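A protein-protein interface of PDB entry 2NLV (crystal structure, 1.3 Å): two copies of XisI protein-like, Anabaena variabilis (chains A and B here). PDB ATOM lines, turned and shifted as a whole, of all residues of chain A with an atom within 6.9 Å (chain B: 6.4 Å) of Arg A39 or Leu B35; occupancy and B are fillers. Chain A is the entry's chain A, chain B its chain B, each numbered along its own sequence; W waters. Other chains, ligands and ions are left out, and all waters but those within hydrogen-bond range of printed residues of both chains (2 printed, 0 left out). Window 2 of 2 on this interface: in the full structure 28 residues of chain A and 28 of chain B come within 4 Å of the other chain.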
ATOM      1  N   ILE A  34      15.673  12.432 -12.681  1.00  0.00           N
ATOM      2  CA  ILE A  34      14.958  11.697 -11.656  1.00  0.00           C
ATOM      3  C   ILE A  34      14.585  12.711 -10.588  1.00  0.00           C
ATOM      4  O   ILE A  34      15.433  13.073  -9.744  1.00  0.00           O
ATOM      5  CB  ILE A  34      15.788  10.541 -11.068  1.00  0.00           C
ATOM      6  CG1 ILE A  34      16.269   9.597 -12.174  1.00  0.00           C
ATOM      7  CG2 ILE A  34      14.966   9.783 -10.028  1.00  0.00           C
ATOM      8  CD1 ILE A  34      17.038   8.439 -11.776  1.00  0.00           C
ATOM      9  N   LEU A  35      13.347  13.152 -10.615  1.00  0.00           N
ATOM     10  CA  LEU A  35      12.907  14.224  -9.765  1.00  0.00           C
ATOM     11  C   LEU A  35      11.753  13.728  -8.919  1.00  0.00           C
ATOM     12  O   LEU A  35      10.631  13.553  -9.407  1.00  0.00           O
ATOM     13  CB  LEU A  35      12.515  15.488 -10.569  1.00  0.00           C
ATOM     14  CG  LEU A  35      13.489  15.925 -11.696  1.00  0.00           C
ATOM     15  CD1 LEU A  35      12.936  16.990 -12.584  1.00  0.00           C
ATOM     16  CD2 LEU A  35      14.865  16.319 -11.101  1.00  0.00           C
ATOM     17  N   ASP A  36      12.017  13.452  -7.653  1.00  0.00           N
ATOM     18  CA  ASP A  36      10.988  13.113  -6.658  1.00  0.00           C
ATOM     19  C   ASP A  36      10.735  14.299  -5.749  1.00  0.00           C
ATOM     20  O   ASP A  36      11.507  14.583  -4.860  1.00  0.00           O
ATOM     21  CB  ASP A  36      11.448  11.875  -5.930  1.00  0.00           C
ATOM     22  CG  ASP A  36      10.510  11.458  -4.853  1.00  0.00           C
ATOM     23  OD1 ASP A  36       9.525  12.184  -4.523  1.00  0.00           O
ATOM     24  OD2 ASP A  36      10.725  10.328  -4.396  1.00  0.00           O
ATOM     25  N   THR A  37       9.646  15.014  -6.003  1.00  0.00           N
ATOM     26  CA  THR A  37       9.332  16.215  -5.248  1.00  0.00           C
ATOM     27  C   THR A  37       8.604  15.947  -3.946  1.00  0.00           C
ATOM     28  O   THR A  37       8.491  16.822  -3.106  1.00  0.00           O
ATOM     29  CB  THR A  37       8.460  17.162  -6.041  1.00  0.00           C
ATOM     30  OG1 THR A  37       7.319  16.450  -6.523  1.00  0.00           O
ATOM     31  CG2 THR A  37       9.269  17.725  -7.214  1.00  0.00           C
ATOM     32  N   GLU A  38       8.080  14.749  -3.793  1.00  0.00           N
ATOM     33  CA  GLU A  38       7.471  14.366  -2.506  1.00  0.00           C
ATOM     34  C   GLU A  38       8.519  14.080  -1.428  1.00  0.00           C
ATOM     35  O   GLU A  38       8.378  14.462  -0.281  1.00  0.00           O
ATOM     36  CB  GLU A  38       6.542  13.173  -2.654  1.00  0.00           C
ATOM     37  CG  GLU A  38       5.334  13.505  -3.518  1.00  0.00           C
ATOM     38  CD  GLU A  38       4.481  14.651  -2.999  1.00  0.00           C
ATOM     39  N   ARG A  39       9.563  13.337  -1.806  1.00  0.00           N
ATOM     40  CA  ARG A  39      10.669  12.957  -0.889  1.00  0.00           C
ATOM     41  C   ARG A  39      11.915  13.829  -1.066  1.00  0.00           C
ATOM     42  O   ARG A  39      12.886  13.722  -0.308  1.00  0.00           O
ATOM     43  CB  ARG A  39      11.057  11.465  -1.003  1.00  0.00           C
ATOM     44  CG  ARG A  39      10.015  10.558  -0.325  1.00  0.00           C
ATOM     45  CD  ARG A  39       9.813   9.197  -1.027  1.00  0.00           C
ATOM     46  NE  ARG A  39       9.193   9.444  -2.316  1.00  0.00           N
ATOM     47  CZ  ARG A  39       7.881   9.513  -2.577  1.00  0.00           C
ATOM     48  NH1 ARG A  39       6.948   9.225  -1.653  1.00  0.00           N
ATOM     49  NH2 ARG A  39       7.460   9.861  -3.776  1.00  0.00           N
ATOM     50  N   ASN A  40      11.877  14.724  -2.033  1.00  0.00           N
ATOM     51  CA  ASN A  40      12.947  15.689  -2.271  1.00  0.00           C
ATOM     52  C   ASN A  40      14.282  15.040  -2.587  1.00  0.00           C
ATOM     53  O   ASN A  40      15.305  15.301  -1.938  1.00  0.00           O
ATOM     54  CB  ASN A  40      13.073  16.654  -1.080  1.00  0.00           C
ATOM     55  CG  ASN A  40      11.952  17.631  -1.054  1.00  0.00           C
ATOM     56  OD1 ASN A  40      11.749  18.383  -2.005  1.00  0.00           O
ATOM     57  ND2 ASN A  40      11.257  17.681   0.056  1.00  0.00           N
ATOM     58  N   HIS A  41      14.254  14.185  -3.613  1.00  0.00           N
ATOM     59  CA  HIS A  41      15.445  13.589  -4.161  1.00  0.00           C
ATOM     60  C   HIS A  41      15.504  13.900  -5.633  1.00  0.00           C
ATOM     61  O   HIS A  41      14.557  13.618  -6.367  1.00  0.00           O
ATOM     62  CB  HIS A  41      15.447  12.052  -3.950  1.00  0.00           C
ATOM     63  CG  HIS A  41      15.251  11.605  -2.537  1.00  0.00           C
ATOM     64  ND1 HIS A  41      16.115  11.923  -1.514  1.00  0.00           N
ATOM     65  CD2 HIS A  41      14.295  10.813  -1.986  1.00  0.00           C
ATOM     66  CE1 HIS A  41      15.695  11.328  -0.402  1.00  0.00           C
ATOM     67  NE2 HIS A  41      14.600  10.640  -0.662  1.00  0.00           N
ATOM     68  N   TYR A  42      16.674  14.385  -6.095  1.00  0.00           N
ATOM     69  CA  TYR A  42      16.777  14.907  -7.436  1.00  0.00           C
ATOM     70  C   TYR A  42      18.096  14.486  -8.060  1.00  0.00           C
ATOM     71  O   TYR A  42      19.151  14.875  -7.536  1.00  0.00           O
ATOM     72  CB  TYR A  42      16.656  16.442  -7.417  1.00  0.00           C
ATOM     73  CG  TYR A  42      15.399  16.961  -6.685  1.00  0.00           C
ATOM     74  CD1 TYR A  42      14.162  17.016  -7.325  1.00  0.00           C
ATOM     75  CD2 TYR A  42      15.446  17.339  -5.337  1.00  0.00           C
ATOM     76  CE1 TYR A  42      13.046  17.490  -6.632  1.00  0.00           C
ATOM     77  CE2 TYR A  42      14.353  17.806  -4.675  1.00  0.00           C
ATOM     78  CZ  TYR A  42      13.173  17.851  -5.333  1.00  0.00           C
ATOM     79  OH  TYR A  42      12.007  18.299  -4.685  1.00  0.00           O
ATOM     80  N   ASP A  63      19.588  16.408  -2.633  1.00  0.00           N
ATOM     81  CA  ASP A  63      18.407  16.198  -1.787  1.00  0.00           C
ATOM     82  C   ASP A  63      18.010  17.515  -1.153  1.00  0.00           C
ATOM     83  O   ASP A  63      18.818  18.409  -1.057  1.00  0.00           O
ATOM     84  CB  ASP A  63      18.672  15.183  -0.719  1.00  0.00           C
ATOM     85  CG  ASP A  63      19.072  13.822  -1.295  1.00  0.00           C
ATOM     86  OD1 ASP A  63      18.339  13.328  -2.189  1.00  0.00           O
ATOM     87  OD2 ASP A  63      20.080  13.279  -0.820  1.00  0.00           O
ATOM     88  N   ILE A  64      16.779  17.612  -0.680  1.00  0.00           N
ATOM     89  CA  ILE A  64      16.387  18.682   0.228  1.00  0.00           C
ATOM     90  C   ILE A  64      15.900  18.019   1.486  1.00  0.00           C
ATOM     91  O   ILE A  64      14.971  17.229   1.455  1.00  0.00           O
ATOM     92  CB  ILE A  64      15.352  19.678  -0.381  1.00  0.00           C
ATOM     93  CG1 ILE A  64      15.817  20.233  -1.712  1.00  0.00           C
ATOM     94  CG2 ILE A  64      15.135  20.816   0.609  1.00  0.00           C
ATOM     95  CD1 ILE A  64      14.757  20.970  -2.515  1.00  0.00           C
ATOM     96  N   LYS A  65      16.628  18.259   2.570  1.00  0.00           N
ATOM     97  CA  LYS A  65      16.447  17.581   3.872  1.00  0.00           C
ATOM     98  C   LYS A  65      16.338  18.629   4.929  1.00  0.00           C
ATOM     99  O   LYS A  65      17.200  19.455   5.071  1.00  0.00           O
ATOM    100  CB  LYS A  65      17.617  16.657   4.199  1.00  0.00           C
ATOM    101  CG  LYS A  65      17.858  15.526   3.208  1.00  0.00           C
ATOM    102  CD  LYS A  65      19.216  14.844   3.396  1.00  0.00           C
ATOM    103  CE  LYS A  65      19.264  14.009   4.675  1.00  0.00           C
ATOM    104  NZ  LYS A  65      20.658  13.671   5.096  1.00  0.00           N
ATOM    105  N   VAL B  12       5.902  -1.741  -8.718  1.00  0.00           N
ATOM    106  CA  VAL B  12       7.300  -1.340  -8.545  1.00  0.00           C
ATOM    107  C   VAL B  12       7.427  -0.556  -7.238  1.00  0.00           C
ATOM    108  O   VAL B  12       8.354  -0.826  -6.472  1.00  0.00           O
ATOM    109  CB  VAL B  12       7.766  -0.523  -9.754  1.00  0.00           C
ATOM    110  CG1 VAL B  12       9.038   0.216  -9.486  1.00  0.00           C
ATOM    111  CG2 VAL B  12       7.952  -1.436 -10.973  1.00  0.00           C
ATOM    112  N   LYS B  13       6.512   0.372  -6.964  1.00  0.00           N
ATOM    113  CA  LYS B  13       6.549   1.100  -5.710  1.00  0.00           C
ATOM    114  C   LYS B  13       6.447   0.183  -4.505  1.00  0.00           C
ATOM    115  O   LYS B  13       7.195   0.352  -3.537  1.00  0.00           O
ATOM    116  CB  LYS B  13       5.475   2.178  -5.657  1.00  0.00           C
ATOM    117  CG  LYS B  13       5.770   3.356  -6.593  1.00  0.00           C
ATOM    118  CD  LYS B  13       4.704   4.455  -6.600  1.00  0.00           C
ATOM    119  CE  LYS B  13       3.645   4.247  -7.591  1.00  0.00           C
ATOM    120  NZ  LYS B  13       2.897   5.526  -7.717  1.00  0.00           N
ATOM    121  N   LEU B  16       9.859  -1.847  -4.100  1.00  0.00           N
ATOM    122  CA  LEU B  16      10.951  -1.008  -3.632  1.00  0.00           C
ATOM    123  C   LEU B  16      10.751  -0.523  -2.219  1.00  0.00           C
ATOM    124  O   LEU B  16      11.689  -0.458  -1.439  1.00  0.00           O
ATOM    125  CB  LEU B  16      11.189   0.177  -4.563  1.00  0.00           C
ATOM    126  CG  LEU B  16      11.822  -0.174  -5.893  1.00  0.00           C
ATOM    127  CD1 LEU B  16      11.891   1.109  -6.715  1.00  0.00           C
ATOM    128  CD2 LEU B  16      13.243  -0.718  -5.735  1.00  0.00           C
ATOM    129  N   THR B  17       9.515  -0.172  -1.892  1.00  0.00           N
ATOM    130  CA  THR B  17       9.198   0.183  -0.520  1.00  0.00           C
ATOM    131  C   THR B  17       9.520  -0.986   0.451  1.00  0.00           C
ATOM    132  O   THR B  17      10.042  -0.749   1.534  1.00  0.00           O
ATOM    133  CB  THR B  17       7.766   0.706  -0.409  1.00  0.00           C
ATOM    134  OG1 THR B  17       7.594   1.826  -1.291  1.00  0.00           O
ATOM    135  CG2 THR B  17       7.438   1.120   1.052  1.00  0.00           C
ATOM    136  N   LEU B  33      14.324   6.253  -0.740  1.00  0.00           N
ATOM    137  CA  LEU B  33      13.363   5.747  -1.679  1.00  0.00           C
ATOM    138  C   LEU B  33      13.039   6.894  -2.612  1.00  0.00           C
ATOM    139  O   LEU B  33      12.604   7.973  -2.176  1.00  0.00           O
ATOM    140  CB  LEU B  33      12.119   5.268  -0.927  1.00  0.00           C
ATOM    141  CG  LEU B  33      11.018   4.609  -1.736  1.00  0.00           C
ATOM    142  CD1 LEU B  33      11.471   3.284  -2.370  1.00  0.00           C
ATOM    143  CD2 LEU B  33       9.738   4.421  -0.856  1.00  0.00           C
ATOM    144  N   ILE B  34      13.219   6.672  -3.903  1.00  0.00           N
ATOM    145  CA  ILE B  34      13.101   7.740  -4.901  1.00  0.00           C
ATOM    146  C   ILE B  34      12.064   7.256  -5.893  1.00  0.00           C
ATOM    147  O   ILE B  34      12.244   6.277  -6.610  1.00  0.00           O
ATOM    148  CB  ILE B  34      14.448   8.009  -5.564  1.00  0.00           C
ATOM    149  CG1 ILE B  34      15.550   8.320  -4.522  1.00  0.00           C
ATOM    150  CG2 ILE B  34      14.282   9.160  -6.567  1.00  0.00           C
ATOM    151  CD1 ILE B  34      16.902   8.698  -5.096  1.00  0.00           C
ATOM    152  N   LEU B  35      10.956   7.971  -5.933  1.00  0.00           N
ATOM    153  CA  LEU B  35       9.850   7.607  -6.794  1.00  0.00           C
ATOM    154  C   LEU B  35       9.509   8.805  -7.686  1.00  0.00           C
ATOM    155  O   LEU B  35       8.863   9.751  -7.230  1.00  0.00           O
ATOM    156  CB  LEU B  35       8.643   7.193  -5.952  1.00  0.00           C
ATOM    157  CG  LEU B  35       8.919   6.191  -4.793  1.00  0.00           C
ATOM    158  CD1 LEU B  35       7.674   6.017  -3.934  1.00  0.00           C
ATOM    159  CD2 LEU B  35       9.440   4.852  -5.340  1.00  0.00           C
ATOM    160  N   ASP B  36       9.897   8.776  -8.933  1.00  0.00           N
ATOM    161  CA  ASP B  36       9.554   9.822  -9.898  1.00  0.00           C
ATOM    162  C   ASP B  36       8.475   9.238 -10.792  1.00  0.00           C
ATOM    163  O   ASP B  36       8.733   8.435 -11.677  1.00  0.00           O
ATOM    164  CB  ASP B  36      10.810  10.218 -10.698  1.00  0.00           C
ATOM    165  CG  ASP B  36      10.528  11.217 -11.788  1.00  0.00           C
ATOM    166  OD1 ASP B  36       9.348  11.430 -12.171  1.00  0.00           O
ATOM    167  OD2 ASP B  36      11.499  11.818 -12.255  1.00  0.00           O
ATOM    168  N   THR B  37       7.243   9.650 -10.512  1.00  0.00           N
ATOM    169  CA  THR B  37       6.094   9.127 -11.228  1.00  0.00           C
ATOM    170  C   THR B  37       5.781   9.837 -12.523  1.00  0.00           C
ATOM    171  O   THR B  37       4.877   9.395 -13.246  1.00  0.00           O
ATOM    172  CB  THR B  37       4.846   9.176 -10.330  1.00  0.00           C
ATOM    173  OG1 THR B  37       4.698  10.487  -9.807  1.00  0.00           O
ATOM    174  CG2 THR B  37       5.029   8.232  -9.148  1.00  0.00           C
ATOM    175  N   GLU B  38       6.500  10.907 -12.837  1.00  0.00           N
ATOM    176  CA  GLU B  38       6.302  11.661 -14.081  1.00  0.00           C
ATOM    177  C   GLU B  38       7.183  11.146 -15.201  1.00  0.00           C
ATOM    178  O   GLU B  38       6.762  11.136 -16.347  1.00  0.00           O
ATOM    179  CB  GLU B  38       6.579  13.137 -13.858  1.00  0.00           C
ATOM    180  CG  GLU B  38       5.704  13.754 -12.801  1.00  0.00           C
ATOM    181  N   HIS B  41      10.902   6.716 -12.986  1.00  0.00           N
ATOM    182  CA  HIS B  41      12.209   6.242 -12.488  1.00  0.00           C
ATOM    183  C   HIS B  41      12.040   6.001 -10.997  1.00  0.00           C
ATOM    184  O   HIS B  41      11.546   6.867 -10.271  1.00  0.00           O
ATOM    185  CB  HIS B  41      13.283   7.301 -12.696  1.00  0.00           C
ATOM    186  CG  HIS B  41      13.418   7.775 -14.100  1.00  0.00           C
ATOM    187  ND1 HIS B  41      13.702   6.926 -15.140  1.00  0.00           N
ATOM    188  CD2 HIS B  41      13.386   9.028 -14.631  1.00  0.00           C
ATOM    189  CE1 HIS B  41      13.849   7.643 -16.255  1.00  0.00           C
ATOM    190  NE2 HIS B  41      13.670   8.913 -15.956  1.00  0.00           N
ATOM    191  N   TYR B  42      12.440   4.799 -10.534  1.00  0.00           N
ATOM    192  CA  TYR B  42      12.176   4.374  -9.163  1.00  0.00           C
ATOM    193  C   TYR B  42      13.412   3.702  -8.622  1.00  0.00           C
ATOM    194  O   TYR B  42      13.967   2.763  -9.219  1.00  0.00           O
ATOM    195  CB  TYR B  42      11.044   3.378  -9.154  1.00  0.00           C
ATOM    196  CG  TYR B  42       9.802   3.932  -9.850  1.00  0.00           C
ATOM    197  CD1 TYR B  42       8.923   4.743  -9.157  1.00  0.00           C
ATOM    198  CD2 TYR B  42       9.507   3.661 -11.203  1.00  0.00           C
ATOM    199  CE1 TYR B  42       7.792   5.313  -9.761  1.00  0.00           C
ATOM    200  CE2 TYR B  42       8.357   4.221 -11.804  1.00  0.00           C
ATOM    201  CZ  TYR B  42       7.525   5.037 -11.067  1.00  0.00           C
ATOM    202  OH  TYR B  42       6.359   5.597 -11.630  1.00  0.00           O
ATOM    203  N   GLN B  43      13.906   4.169  -7.475  1.00  0.00           N
ATOM    204  CA  GLN B  43      15.176   3.718  -6.935  1.00  0.00           C
ATOM    205  C   GLN B  43      15.127   3.507  -5.424  1.00  0.00           C
ATOM    206  O   GLN B  43      14.374   4.174  -4.702  1.00  0.00           O
ATOM    207  CB  GLN B  43      16.268   4.753  -7.189  1.00  0.00           C
ATOM    208  CG  GLN B  43      16.595   5.036  -8.633  1.00  0.00           C
ATOM    209  CD  GLN B  43      17.481   6.195  -8.754  1.00  0.00           C
ATOM    210  OE1 GLN B  43      18.628   6.092  -9.294  1.00  0.00           O
ATOM    211  NE2 GLN B  43      17.021   7.332  -8.310  1.00  0.00           N
HETATM  212  O   HOH W   1      13.574   8.636   0.996  1.00  0.00           O
HETATM  213  O   HOH W   2       7.471  12.678  -9.841  1.00  0.00           O
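Of the 12 printed residues of chain A, 5 touch a printed residue of chain B.
Hydrophobic or aromatic side chains of chain A that line the printed part of chain B: Ile A34 and His A41.
Among the printed residues, no Asp or Glu carboxylate lies within 4 Å of a Lys or Arg side-chain nitrogen of the other chain.
Ile A34 touches its own counterpart, Ile B34.
Ile A34 touches Asp B36, and with the chains exchanged Asp A36 touches Ile B34.
Ile A34 touches His B41, and with the chains exchanged His A41 touches Ile B34.
Leu A35 touches Asp B36, and with the chains exchanged Asp A36 touches Leu B35.
Positions printed for both chains: 34, 35, 36, 37, 38, 41 and 42.
Water W1 lies within hydrogen-bond range of a ring nitrogen (NE2) of His A41 (2.8 Å) and the backbone NH (N) of Leu B33 (3.0 Å).
Water W2 lies within hydrogen-bond range of the backbone NH (N) of Thr B37, the side-chain carboxylate (OD1) of Asp B36 and the backbone carbonyl oxygen (O) of Leu A35.
Among the printed residues, pairs that only touch across the chains: Arg A39 with Leu B33, His A41 with Leu B33, Ile A34 with Asp B36, Asp A36 with Ile B34, Ile A34 with Ile B34, Ile A34 with Gln B43, Arg A39 with Leu B35, Asp A36 with Leu B33, His A41 with Ile B34 and Ile A34 with His B41.
Of the printed residues of chain B, Ile A34 touches Ile B34, Asp B36, His B41 and Gln B43.
Of the printed residues of chain B, Leu A35 touches Asp B36.
Of the printed residues of chain B, Asp A36 touches Leu B33, Ile B34 and Leu B35.
Printed residues of chain B within 4 Å of Arg A39: Leu B33 (3.3 Å) and Leu B35 (3.6 Å).
Of the printed residues of chain A, Asp B36 touches Ile A34 (3.5 Å) and Leu A35 (2.8 Å).
Printed residues of chain A within 4 Å of Gln B43: Ile A34.
The nearest printed residue of chain B that does not touch Arg A39 is Ile B34 (5.0 Å).
ND1 of His A41 sits at hydrogen-bond distance from OD1 of Asp A63, at 2.7 Å.
The backbone NH (N) of Glu B38 is in hydrogen-bond range of the side-chain carboxylate (OD1) of Asp B36, 3.0 Å away.
N of Asp A36 lies within hydrogen-bond range of O of His A41, 2.9 Å away.
OD1 of Asp A36 is in hydrogen-bond range of N of Glu A38 (3.0 Å).
The backbone NH of Asp B36 sits at hydrogen-bond distance from the backbone carbonyl oxygen of His B41.
The side-chain carboxylate (OD2) of Asp A36 is in salt-bridge range of the guanidinium group (NE) of Arg A39 (2.7 Å).
The side-chain carboxylate (OD2) of Asp A36 lies within hydrogen-bond range of the backbone NH (N) of Leu B35.
The side-chain carboxylate (OD2) of Asp B36 is in hydrogen-bond range of the backbone NH (N) of Leu A35 (2.8 Å).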
